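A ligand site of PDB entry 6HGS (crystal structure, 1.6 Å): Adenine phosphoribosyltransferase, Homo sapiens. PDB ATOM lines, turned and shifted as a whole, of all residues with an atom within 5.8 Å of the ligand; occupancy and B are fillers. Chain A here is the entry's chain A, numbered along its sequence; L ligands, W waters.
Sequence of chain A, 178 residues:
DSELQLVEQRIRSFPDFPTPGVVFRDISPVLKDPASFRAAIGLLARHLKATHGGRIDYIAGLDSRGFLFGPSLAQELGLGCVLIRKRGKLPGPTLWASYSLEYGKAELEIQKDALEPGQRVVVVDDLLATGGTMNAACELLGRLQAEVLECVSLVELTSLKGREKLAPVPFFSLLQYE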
ATOM      1  N   VAL A  23       0.924 -13.496  20.475  1.00  0.00           N
ATOM      2  CA  VAL A  23       0.731 -12.182  21.064  1.00  0.00           C
ATOM      3  C   VAL A  23       0.253 -12.361  22.477  1.00  0.00           C
ATOM      4  O   VAL A  23      -0.833 -12.885  22.706  1.00  0.00           O
ATOM      5  CB  VAL A  23      -0.280 -11.341  20.272  1.00  0.00           C
ATOM      6  CG1 VAL A  23      -0.432  -9.972  20.886  1.00  0.00           C
ATOM      7  CG2 VAL A  23       0.140 -11.238  18.809  1.00  0.00           C
ATOM      8  N   PHE A  24       1.070 -11.933  23.428  1.00  0.00           N
ATOM      9  CA  PHE A  24       0.705 -12.012  24.823  1.00  0.00           C
ATOM     10  C   PHE A  24      -0.241 -10.887  25.150  1.00  0.00           C
ATOM     11  O   PHE A  24       0.032  -9.736  24.836  1.00  0.00           O
ATOM     12  CB  PHE A  24       1.947 -11.921  25.695  1.00  0.00           C
ATOM     13  CG  PHE A  24       1.668 -12.169  27.160  1.00  0.00           C
ATOM     14  CD1 PHE A  24       1.686 -13.450  27.675  1.00  0.00           C
ATOM     15  CD2 PHE A  24       1.371 -11.117  28.007  1.00  0.00           C
ATOM     16  CE1 PHE A  24       1.422 -13.685  29.002  1.00  0.00           C
ATOM     17  CE2 PHE A  24       1.124 -11.349  29.351  1.00  0.00           C
ATOM     18  CZ  PHE A  24       1.136 -12.630  29.842  1.00  0.00           C
ATOM     19  N   ARG A  25      -1.386 -11.215  25.749  1.00  0.00           N
ATOM     20  CA  ARG A  25      -2.341 -10.215  26.194  1.00  0.00           C
ATOM     21  C   ARG A  25      -2.114  -9.923  27.681  1.00  0.00           C
ATOM     22  O   ARG A  25      -2.347 -10.786  28.544  1.00  0.00           O
ATOM     23  CB  ARG A  25      -3.777 -10.679  25.937  1.00  0.00           C
ATOM     24  CG  ARG A  25      -4.029 -11.158  24.511  1.00  0.00           C
ATOM     25  CD  ARG A  25      -3.873 -10.050  23.492  1.00  0.00           C
ATOM     26  NE  ARG A  25      -4.037 -10.571  22.132  1.00  0.00           N
ATOM     27  CZ  ARG A  25      -4.212  -9.806  21.055  1.00  0.00           C
ATOM     28  NH1 ARG A  25      -4.274  -8.492  21.173  1.00  0.00           N
ATOM     29  NH2 ARG A  25      -4.347 -10.366  19.863  1.00  0.00           N
ATOM     30  N   ASP A  26      -1.634  -8.722  27.968  1.00  0.00           N
ATOM     31  CA  ASP A  26      -1.244  -8.321  29.328  1.00  0.00           C
ATOM     32  C   ASP A  26      -2.433  -7.640  29.986  1.00  0.00           C
ATOM     33  O   ASP A  26      -2.901  -6.607  29.493  1.00  0.00           O
ATOM     34  CB  ASP A  26      -0.058  -7.366  29.243  1.00  0.00           C
ATOM     35  CG  ASP A  26       0.383  -6.829  30.600  1.00  0.00           C
ATOM     36  OD1 ASP A  26       0.069  -7.459  31.619  1.00  0.00           O
ATOM     37  OD2 ASP A  26       1.063  -5.786  30.601  1.00  0.00           O
ATOM     38  N   ILE A  27      -2.927  -8.216  31.074  1.00  0.00           N
ATOM     39  CA  ILE A  27      -4.054  -7.626  31.802  1.00  0.00           C
ATOM     40  C   ILE A  27      -3.593  -6.736  32.965  1.00  0.00           C
ATOM     41  O   ILE A  27      -4.426  -6.132  33.648  1.00  0.00           O
ATOM     42  CB  ILE A  27      -5.065  -8.694  32.299  1.00  0.00           C
ATOM     43  CG1 ILE A  27      -4.368  -9.812  33.082  1.00  0.00           C
ATOM     44  CG2 ILE A  27      -5.793  -9.303  31.107  1.00  0.00           C
ATOM     45  CD1 ILE A  27      -3.742  -9.361  34.390  1.00  0.00           C
ATOM     46  N   LEU A  62      -7.744 -19.555  40.045  1.00  0.00           N
ATOM     47  CA  LEU A  62      -6.564 -20.312  39.586  1.00  0.00           C
ATOM     48  C   LEU A  62      -5.236 -19.557  39.772  1.00  0.00           C
ATOM     49  O   LEU A  62      -5.105 -18.413  39.401  1.00  0.00           O
ATOM     50  CB  LEU A  62      -6.723 -20.708  38.129  1.00  0.00           C
ATOM     51  CG  LEU A  62      -7.998 -21.458  37.753  1.00  0.00           C
ATOM     52  CD1 LEU A  62      -7.883 -22.041  36.340  1.00  0.00           C
ATOM     53  CD2 LEU A  62      -8.295 -22.564  38.766  1.00  0.00           C
ATOM     54  N   ASP A  63      -4.257 -20.230  40.357  1.00  0.00           N
ATOM     55  CA  ASP A  63      -2.901 -19.701  40.573  1.00  0.00           C
ATOM     56  C   ASP A  63      -2.235 -19.461  39.218  1.00  0.00           C
ATOM     57  O   ASP A  63      -2.279 -20.334  38.366  1.00  0.00           O
ATOM     58  CB  ASP A  63      -2.136 -20.811  41.316  1.00  0.00           C
ATOM     59  CG  ASP A  63      -0.851 -20.368  41.974  1.00  0.00           C
ATOM     60  OD1 ASP A  63      -0.422 -19.212  41.831  1.00  0.00           O
ATOM     61  OD2 ASP A  63      -0.240 -21.246  42.654  1.00  0.00           O
ATOM     62  N   ARG A  65      -2.716 -15.779  38.265  1.00  0.00           N
ATOM     63  CA  ARG A  65      -3.431 -14.553  37.873  1.00  0.00           C
ATOM     64  C   ARG A  65      -4.940 -14.641  38.095  1.00  0.00           C
ATOM     65  O   ARG A  65      -5.608 -13.613  38.239  1.00  0.00           O
ATOM     66  CB  ARG A  65      -3.063 -14.142  36.439  1.00  0.00           C
ATOM     67  CG  ARG A  65      -1.652 -13.612  36.337  1.00  0.00           C
ATOM     68  CD  ARG A  65      -1.384 -12.929  35.006  1.00  0.00           C
ATOM     69  NE  ARG A  65      -1.262 -13.895  33.916  1.00  0.00           N
ATOM     70  CZ  ARG A  65      -0.122 -14.492  33.584  1.00  0.00           C
ATOM     71  NH1 ARG A  65       0.995 -14.233  34.252  1.00  0.00           N
ATOM     72  NH2 ARG A  65      -0.099 -15.356  32.581  1.00  0.00           N
ATOM     73  N   TYR A  99      -1.186 -31.291  32.994  1.00  0.00           N
ATOM     74  CA  TYR A  99      -1.654 -30.825  31.708  1.00  0.00           C
ATOM     75  C   TYR A  99      -0.427 -30.230  31.044  1.00  0.00           C
ATOM     76  O   TYR A  99       0.558 -29.944  31.721  1.00  0.00           O
ATOM     77  CB  TYR A  99      -2.751 -29.769  31.879  1.00  0.00           C
ATOM     78  CG  TYR A  99      -2.266 -28.534  32.571  1.00  0.00           C
ATOM     79  CD1 TYR A  99      -2.090 -28.498  33.943  1.00  0.00           C
ATOM     80  CD2 TYR A  99      -1.931 -27.387  31.836  1.00  0.00           C
ATOM     81  CE1 TYR A  99      -1.625 -27.365  34.591  1.00  0.00           C
ATOM     82  CE2 TYR A  99      -1.464 -26.249  32.475  1.00  0.00           C
ATOM     83  CZ  TYR A  99      -1.311 -26.247  33.848  1.00  0.00           C
ATOM     84  OH  TYR A  99      -0.837 -25.132  34.489  1.00  0.00           O
ATOM     85  N   SER A 100      -0.446 -30.072  29.733  1.00  0.00           N
ATOM     86  CA  SER A 100       0.703 -29.543  29.020  1.00  0.00           C
ATOM     87  C   SER A 100       0.687 -28.017  29.024  1.00  0.00           C
ATOM     88  O   SER A 100      -0.351 -27.404  28.761  1.00  0.00           O
ATOM     89  CB  SER A 100       0.724 -30.061  27.586  1.00  0.00           C
ATOM     90  OG  SER A 100      -0.561 -29.966  26.991  1.00  0.00           O
ATOM     91  N   LEU A 101       1.828 -27.419  29.343  1.00  0.00           N
ATOM     92  CA  LEU A 101       2.040 -25.990  29.279  1.00  0.00           C
ATOM     93  C   LEU A 101       3.229 -25.782  28.358  1.00  0.00           C
ATOM     94  O   LEU A 101       4.239 -26.474  28.509  1.00  0.00           O
ATOM     95  CB  LEU A 101       2.355 -25.435  30.665  1.00  0.00           C
ATOM     96  CG  LEU A 101       2.730 -23.948  30.800  1.00  0.00           C
ATOM     97  CD1 LEU A 101       4.005 -23.608  30.042  1.00  0.00           C
ATOM     98  CD2 LEU A 101       1.573 -23.065  30.350  1.00  0.00           C
ATOM     99  N   ASP A 125     -10.208 -17.436  35.814  1.00  0.00           N
ATOM    100  CA  ASP A 125      -8.802 -17.178  35.497  1.00  0.00           C
ATOM    101  C   ASP A 125      -8.765 -15.905  34.660  1.00  0.00           C
ATOM    102  O   ASP A 125      -9.812 -15.407  34.224  1.00  0.00           O
ATOM    103  CB  ASP A 125      -8.190 -18.353  34.723  1.00  0.00           C
ATOM    104  CG  ASP A 125      -6.661 -18.479  34.888  1.00  0.00           C
ATOM    105  OD1 ASP A 125      -6.035 -17.604  35.544  1.00  0.00           O
ATOM    106  OD2 ASP A 125      -6.090 -19.444  34.323  1.00  0.00           O
ATOM    107  N   ASP A 126      -7.577 -15.362  34.439  1.00  0.00           N
ATOM    108  CA  ASP A 126      -7.485 -14.134  33.671  1.00  0.00           C
ATOM    109  C   ASP A 126      -7.758 -14.351  32.189  1.00  0.00           C
ATOM    110  O   ASP A 126      -8.443 -13.543  31.562  1.00  0.00           O
ATOM    111  CB  ASP A 126      -6.150 -13.393  33.931  1.00  0.00           C
ATOM    112  CG  ASP A 126      -4.907 -14.163  33.455  1.00  0.00           C
ATOM    113  OD1 ASP A 126      -4.924 -15.422  33.406  1.00  0.00           O
ATOM    114  OD2 ASP A 126      -3.876 -13.483  33.201  1.00  0.00           O
ATOM    115  N   LEU A 127      -7.257 -15.432  31.632  1.00  0.00           N
ATOM    116  CA  LEU A 127      -7.302 -15.635  30.192  1.00  0.00           C
ATOM    117  C   LEU A 127      -7.405 -17.124  29.886  1.00  0.00           C
ATOM    118  O   LEU A 127      -6.768 -17.951  30.551  1.00  0.00           O
ATOM    119  CB  LEU A 127      -6.064 -15.010  29.534  1.00  0.00           C
ATOM    120  CG  LEU A 127      -5.912 -15.205  28.015  1.00  0.00           C
ATOM    121  CD1 LEU A 127      -5.168 -14.053  27.390  1.00  0.00           C
ATOM    122  CD2 LEU A 127      -5.234 -16.520  27.685  1.00  0.00           C
ATOM    123  N   LEU A 128      -8.239 -17.448  28.904  1.00  0.00           N
ATOM    124  CA  LEU A 128      -8.363 -18.801  28.366  1.00  0.00           C
ATOM    125  C   LEU A 128      -7.660 -18.881  27.007  1.00  0.00           C
ATOM    126  O   LEU A 128      -7.967 -18.124  26.104  1.00  0.00           O
ATOM    127  CB  LEU A 128      -9.833 -19.164  28.175  1.00  0.00           C
ATOM    128  CG  LEU A 128     -10.101 -20.590  27.672  1.00  0.00           C
ATOM    129  CD1 LEU A 128     -10.068 -21.547  28.839  1.00  0.00           C
ATOM    130  CD2 LEU A 128     -11.440 -20.643  26.969  1.00  0.00           C
ATOM    131  N   ALA A 129      -6.703 -19.797  26.888  1.00  0.00           N
ATOM    132  CA  ALA A 129      -6.009 -20.021  25.638  1.00  0.00           C
ATOM    133  C   ALA A 129      -6.343 -21.420  25.123  1.00  0.00           C
ATOM    134  O   ALA A 129      -7.439 -21.632  24.654  1.00  0.00           O
ATOM    135  CB  ALA A 129      -4.517 -19.817  25.811  1.00  0.00           C
ATOM    136  N   THR A 130      -5.448 -22.386  25.284  1.00  0.00           N
ATOM    137  CA  THR A 130      -5.745 -23.761  24.858  1.00  0.00           C
ATOM    138  C   THR A 130      -6.818 -24.404  25.734  1.00  0.00           C
ATOM    139  O   THR A 130      -7.447 -25.396  25.338  1.00  0.00           O
ATOM    140  CB  THR A 130      -4.515 -24.689  24.926  1.00  0.00           C
ATOM    141  OG1 THR A 130      -4.131 -24.889  26.281  1.00  0.00           O
ATOM    142  CG2 THR A 130      -3.348 -24.116  24.124  1.00  0.00           C
ATOM    143  N   GLY A 131      -6.985 -23.889  26.944  1.00  0.00           N
ATOM    144  CA  GLY A 131      -7.961 -24.450  27.882  1.00  0.00           C
ATOM    145  C   GLY A 131      -7.373 -25.520  28.791  1.00  0.00           C
ATOM    146  O   GLY A 131      -8.087 -26.091  29.619  1.00  0.00           O
ATOM    147  N   GLY A 132      -6.077 -25.784  28.645  1.00  0.00           N
ATOM    148  CA  GLY A 132      -5.428 -26.831  29.442  1.00  0.00           C
ATOM    149  C   GLY A 132      -5.508 -26.556  30.936  1.00  0.00           C
ATOM    150  O   GLY A 132      -5.805 -27.455  31.734  1.00  0.00           O
ATOM    151  N   THR A 133      -5.234 -25.313  31.315  1.00  0.00           N
ATOM    152  CA  THR A 133      -5.230 -24.927  32.722  1.00  0.00           C
ATOM    153  C   THR A 133      -6.632 -25.042  33.316  1.00  0.00           C
ATOM    154  O   THR A 133      -6.829 -25.658  34.377  1.00  0.00           O
ATOM    155  CB  THR A 133      -4.699 -23.493  32.875  1.00  0.00           C
ATOM    156  OG1 THR A 133      -3.393 -23.406  32.293  1.00  0.00           O
ATOM    157  CG2 THR A 133      -4.628 -23.081  34.321  1.00  0.00           C
ATOM    158  N   MET A 134      -7.612 -24.459  32.641  1.00  0.00           N
ATOM    159  CA  MET A 134      -8.980 -24.509  33.126  1.00  0.00           C
ATOM    160  C   MET A 134      -9.518 -25.944  33.131  1.00  0.00           C
ATOM    161  O   MET A 134     -10.278 -26.314  34.026  1.00  0.00           O
ATOM    162  CB  MET A 134      -9.861 -23.632  32.242  1.00  0.00           C
ATOM    163  CG  MET A 134     -11.217 -23.324  32.817  1.00  0.00           C
ATOM    164  SD  MET A 134     -11.109 -22.089  34.111  1.00  0.00           S
ATOM    165  CE  MET A 134     -10.944 -20.583  33.167  1.00  0.00           C
ATOM    166  N   LEU A 157      -8.809 -16.470  23.785  1.00  0.00           N
ATOM    167  CA  LEU A 157      -8.143 -16.512  22.483  1.00  0.00           C
ATOM    168  C   LEU A 157      -8.820 -17.575  21.622  1.00  0.00           C
ATOM    169  O   LEU A 157      -8.556 -18.771  21.742  1.00  0.00           O
ATOM    170  CB  LEU A 157      -6.639 -16.793  22.668  1.00  0.00           C
ATOM    171  CG  LEU A 157      -5.962 -15.848  23.654  1.00  0.00           C
ATOM    172  CD1 LEU A 157      -4.491 -16.207  23.816  1.00  0.00           C
ATOM    173  CD2 LEU A 157      -6.137 -14.398  23.247  1.00  0.00           C
ATOM    174  N   LEU A 160      -7.723 -20.810  19.517  1.00  0.00           N
ATOM    175  CA  LEU A 160      -7.136 -21.955  20.218  1.00  0.00           C
ATOM    176  C   LEU A 160      -8.203 -22.939  20.722  1.00  0.00           C
ATOM    177  O   LEU A 160      -7.872 -24.010  21.225  1.00  0.00           O
ATOM    178  CB  LEU A 160      -6.261 -21.487  21.382  1.00  0.00           C
ATOM    179  CG  LEU A 160      -5.033 -20.660  20.992  1.00  0.00           C
ATOM    180  CD1 LEU A 160      -4.182 -20.379  22.218  1.00  0.00           C
ATOM    181  CD2 LEU A 160      -4.204 -21.375  19.924  1.00  0.00           C
HETATM  182  P1  LIG L   1      -4.137 -22.307  28.618  1.00  0.00           P
HETATM  183  O1  LIG L   1      -3.812 -23.309  29.721  1.00  0.00           O
HETATM  184  O2  LIG L   1      -5.613 -22.015  28.455  1.00  0.00           O
HETATM  185  O3  LIG L   1      -3.455 -22.602  27.285  1.00  0.00           O
HETATM  186  O4  LIG L   1      -3.438 -20.940  29.067  1.00  0.00           O
HETATM  187  C1  LIG L   1      -4.064 -20.056  29.978  1.00  0.00           C
HETATM  188  C2  LIG L   1      -3.210 -19.959  31.215  1.00  0.00           C
HETATM  189  O5  LIG L   1      -1.898 -19.461  30.906  1.00  0.00           O
HETATM  190  C3  LIG L   1      -3.845 -18.981  32.159  1.00  0.00           C
HETATM  191  O6  LIG L   1      -3.587 -19.390  33.508  1.00  0.00           O
HETATM  192  C4  LIG L   1      -3.169 -17.663  31.829  1.00  0.00           C
HETATM  193  O7  LIG L   1      -2.857 -16.973  33.055  1.00  0.00           O
HETATM  194  C5  LIG L   1      -1.888 -18.036  31.070  1.00  0.00           C
HETATM  195  N1  LIG L   1      -1.776 -17.391  29.745  1.00  0.00           N
HETATM  196  C6  LIG L   1      -1.487 -17.974  28.561  1.00  0.00           C
HETATM  197  N2  LIG L   1      -1.428 -17.043  27.559  1.00  0.00           N
HETATM  198  C7  LIG L   1      -1.649 -15.839  28.145  1.00  0.00           C
HETATM  199  C8  LIG L   1      -1.729 -14.441  27.687  1.00  0.00           C
HETATM  200  O8  LIG L   1      -1.560 -14.141  26.474  1.00  0.00           O
HETATM  201  N3  LIG L   1      -1.997 -13.504  28.607  1.00  0.00           N
HETATM  202  C9  LIG L   1      -2.213 -13.810  29.921  1.00  0.00           C
HETATM  203  N4  LIG L   1      -2.485 -12.788  30.781  1.00  0.00           N
HETATM  204  N5  LIG L   1      -2.139 -15.069  30.413  1.00  0.00           N
HETATM  205  C10 LIG L   1      -1.884 -16.059  29.486  1.00  0.00           C
HETATM  206  O   HOH W   1      -1.280 -10.314  32.226  1.00  0.00           O
HETATM  207  O   HOH W   2      -7.138 -22.605  30.571  1.00  0.00           O
HETATM  208  O   HOH W   3      -0.928 -15.595  24.078  1.00  0.00           O
HETATM  209  O   HOH W   4      -1.769 -25.064  29.423  1.00  0.00           O
HETATM  210  O   HOH W   5      -1.071 -18.376  24.803  1.00  0.00           O
HETATM  211  O   HOH W   6      -3.698 -17.982  36.410  1.00  0.00           O
HETATM  212  O   HOH W   7      -1.181 -21.318  26.215  1.00  0.00           O
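O3 of the ligand is in hydrogen-bond range of OG1 of Thr 130 (2.6 Å).
A nitrogen (N3) of the ligand is in hydrogen-bond range of the backbone carbonyl oxygen (O) of Arg 25, at 2.7 Å.
O8 of the ligand sits at hydrogen-bond distance from N of Arg 25.
OG1 of Thr 133 is in hydrogen-bond range of O1 of the ligand (2.6 Å).
The backbone NH of Gly 131 is in hydrogen-bond range of an oxygen (O2) of the ligand, at 2.8 Å.
N5 of the ligand is in hydrogen-bond range of NH2 of Arg 65.
The side-chain carboxylate of Asp 125 lies within hydrogen-bond range of an oxygen (O6) of the ligand (2.6 Å).
N of Ala 129 is in hydrogen-bond range of O2 of the ligand.
The backbone NH of Thr 133 sits at hydrogen-bond distance from an oxygen (O1) of the ligand, at 2.9 Å.
N of Thr 130 lies within hydrogen-bond range of O3 of the ligand, 2.8 Å away.
An oxygen (O7) of the ligand lies within hydrogen-bond range of the side-chain carboxylate (OD1) of Asp 126 (2.6 Å).
OD2 of Asp 126 is in salt-bridge range of NE of Arg 65, 2.7 Å away.
The side-chain hydroxyl (OG1) of Thr 130 lies within hydrogen-bond range of the backbone NH (N) of Gly 132 (3.2 Å).
Merely in contact with the ligand: Phe 24, Leu 127 and Gly 132.
Hydrophobic or aromatic side chains that line the ligand: Phe 24, Leu 127 and Ala 129.
11 residues have an atom within 4 Å of the ligand: Phe 24, Arg 25, Arg 65, Asp 125, Asp 126, Leu 127, Ala 129, Thr 130, Gly 131, Gly 132 and Thr 133.
Water W2 lies within hydrogen-bond range of an oxygen (O2) of the ligand (2.7 Å), the backbone NH (N) of Met 134 (2.8 Å) and the backbone NH (N) of Thr 133 (3.4 Å).
Water W4 lies within hydrogen-bond range of an oxygen (O1) of the ligand and the backbone carbonyl oxygen (O) of Ser 100.
Water W3 bridges O8 of the ligand (2.9 Å) and O of Val 23 (3.0 Å).
Water W1 lies within hydrogen-bond range of the backbone NH (N) of Ile 27 (2.9 Å), a nitrogen (N4) of the ligand (3.1 Å) and the side-chain carboxylate (OD1) of Asp 26 (3.2 Å).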
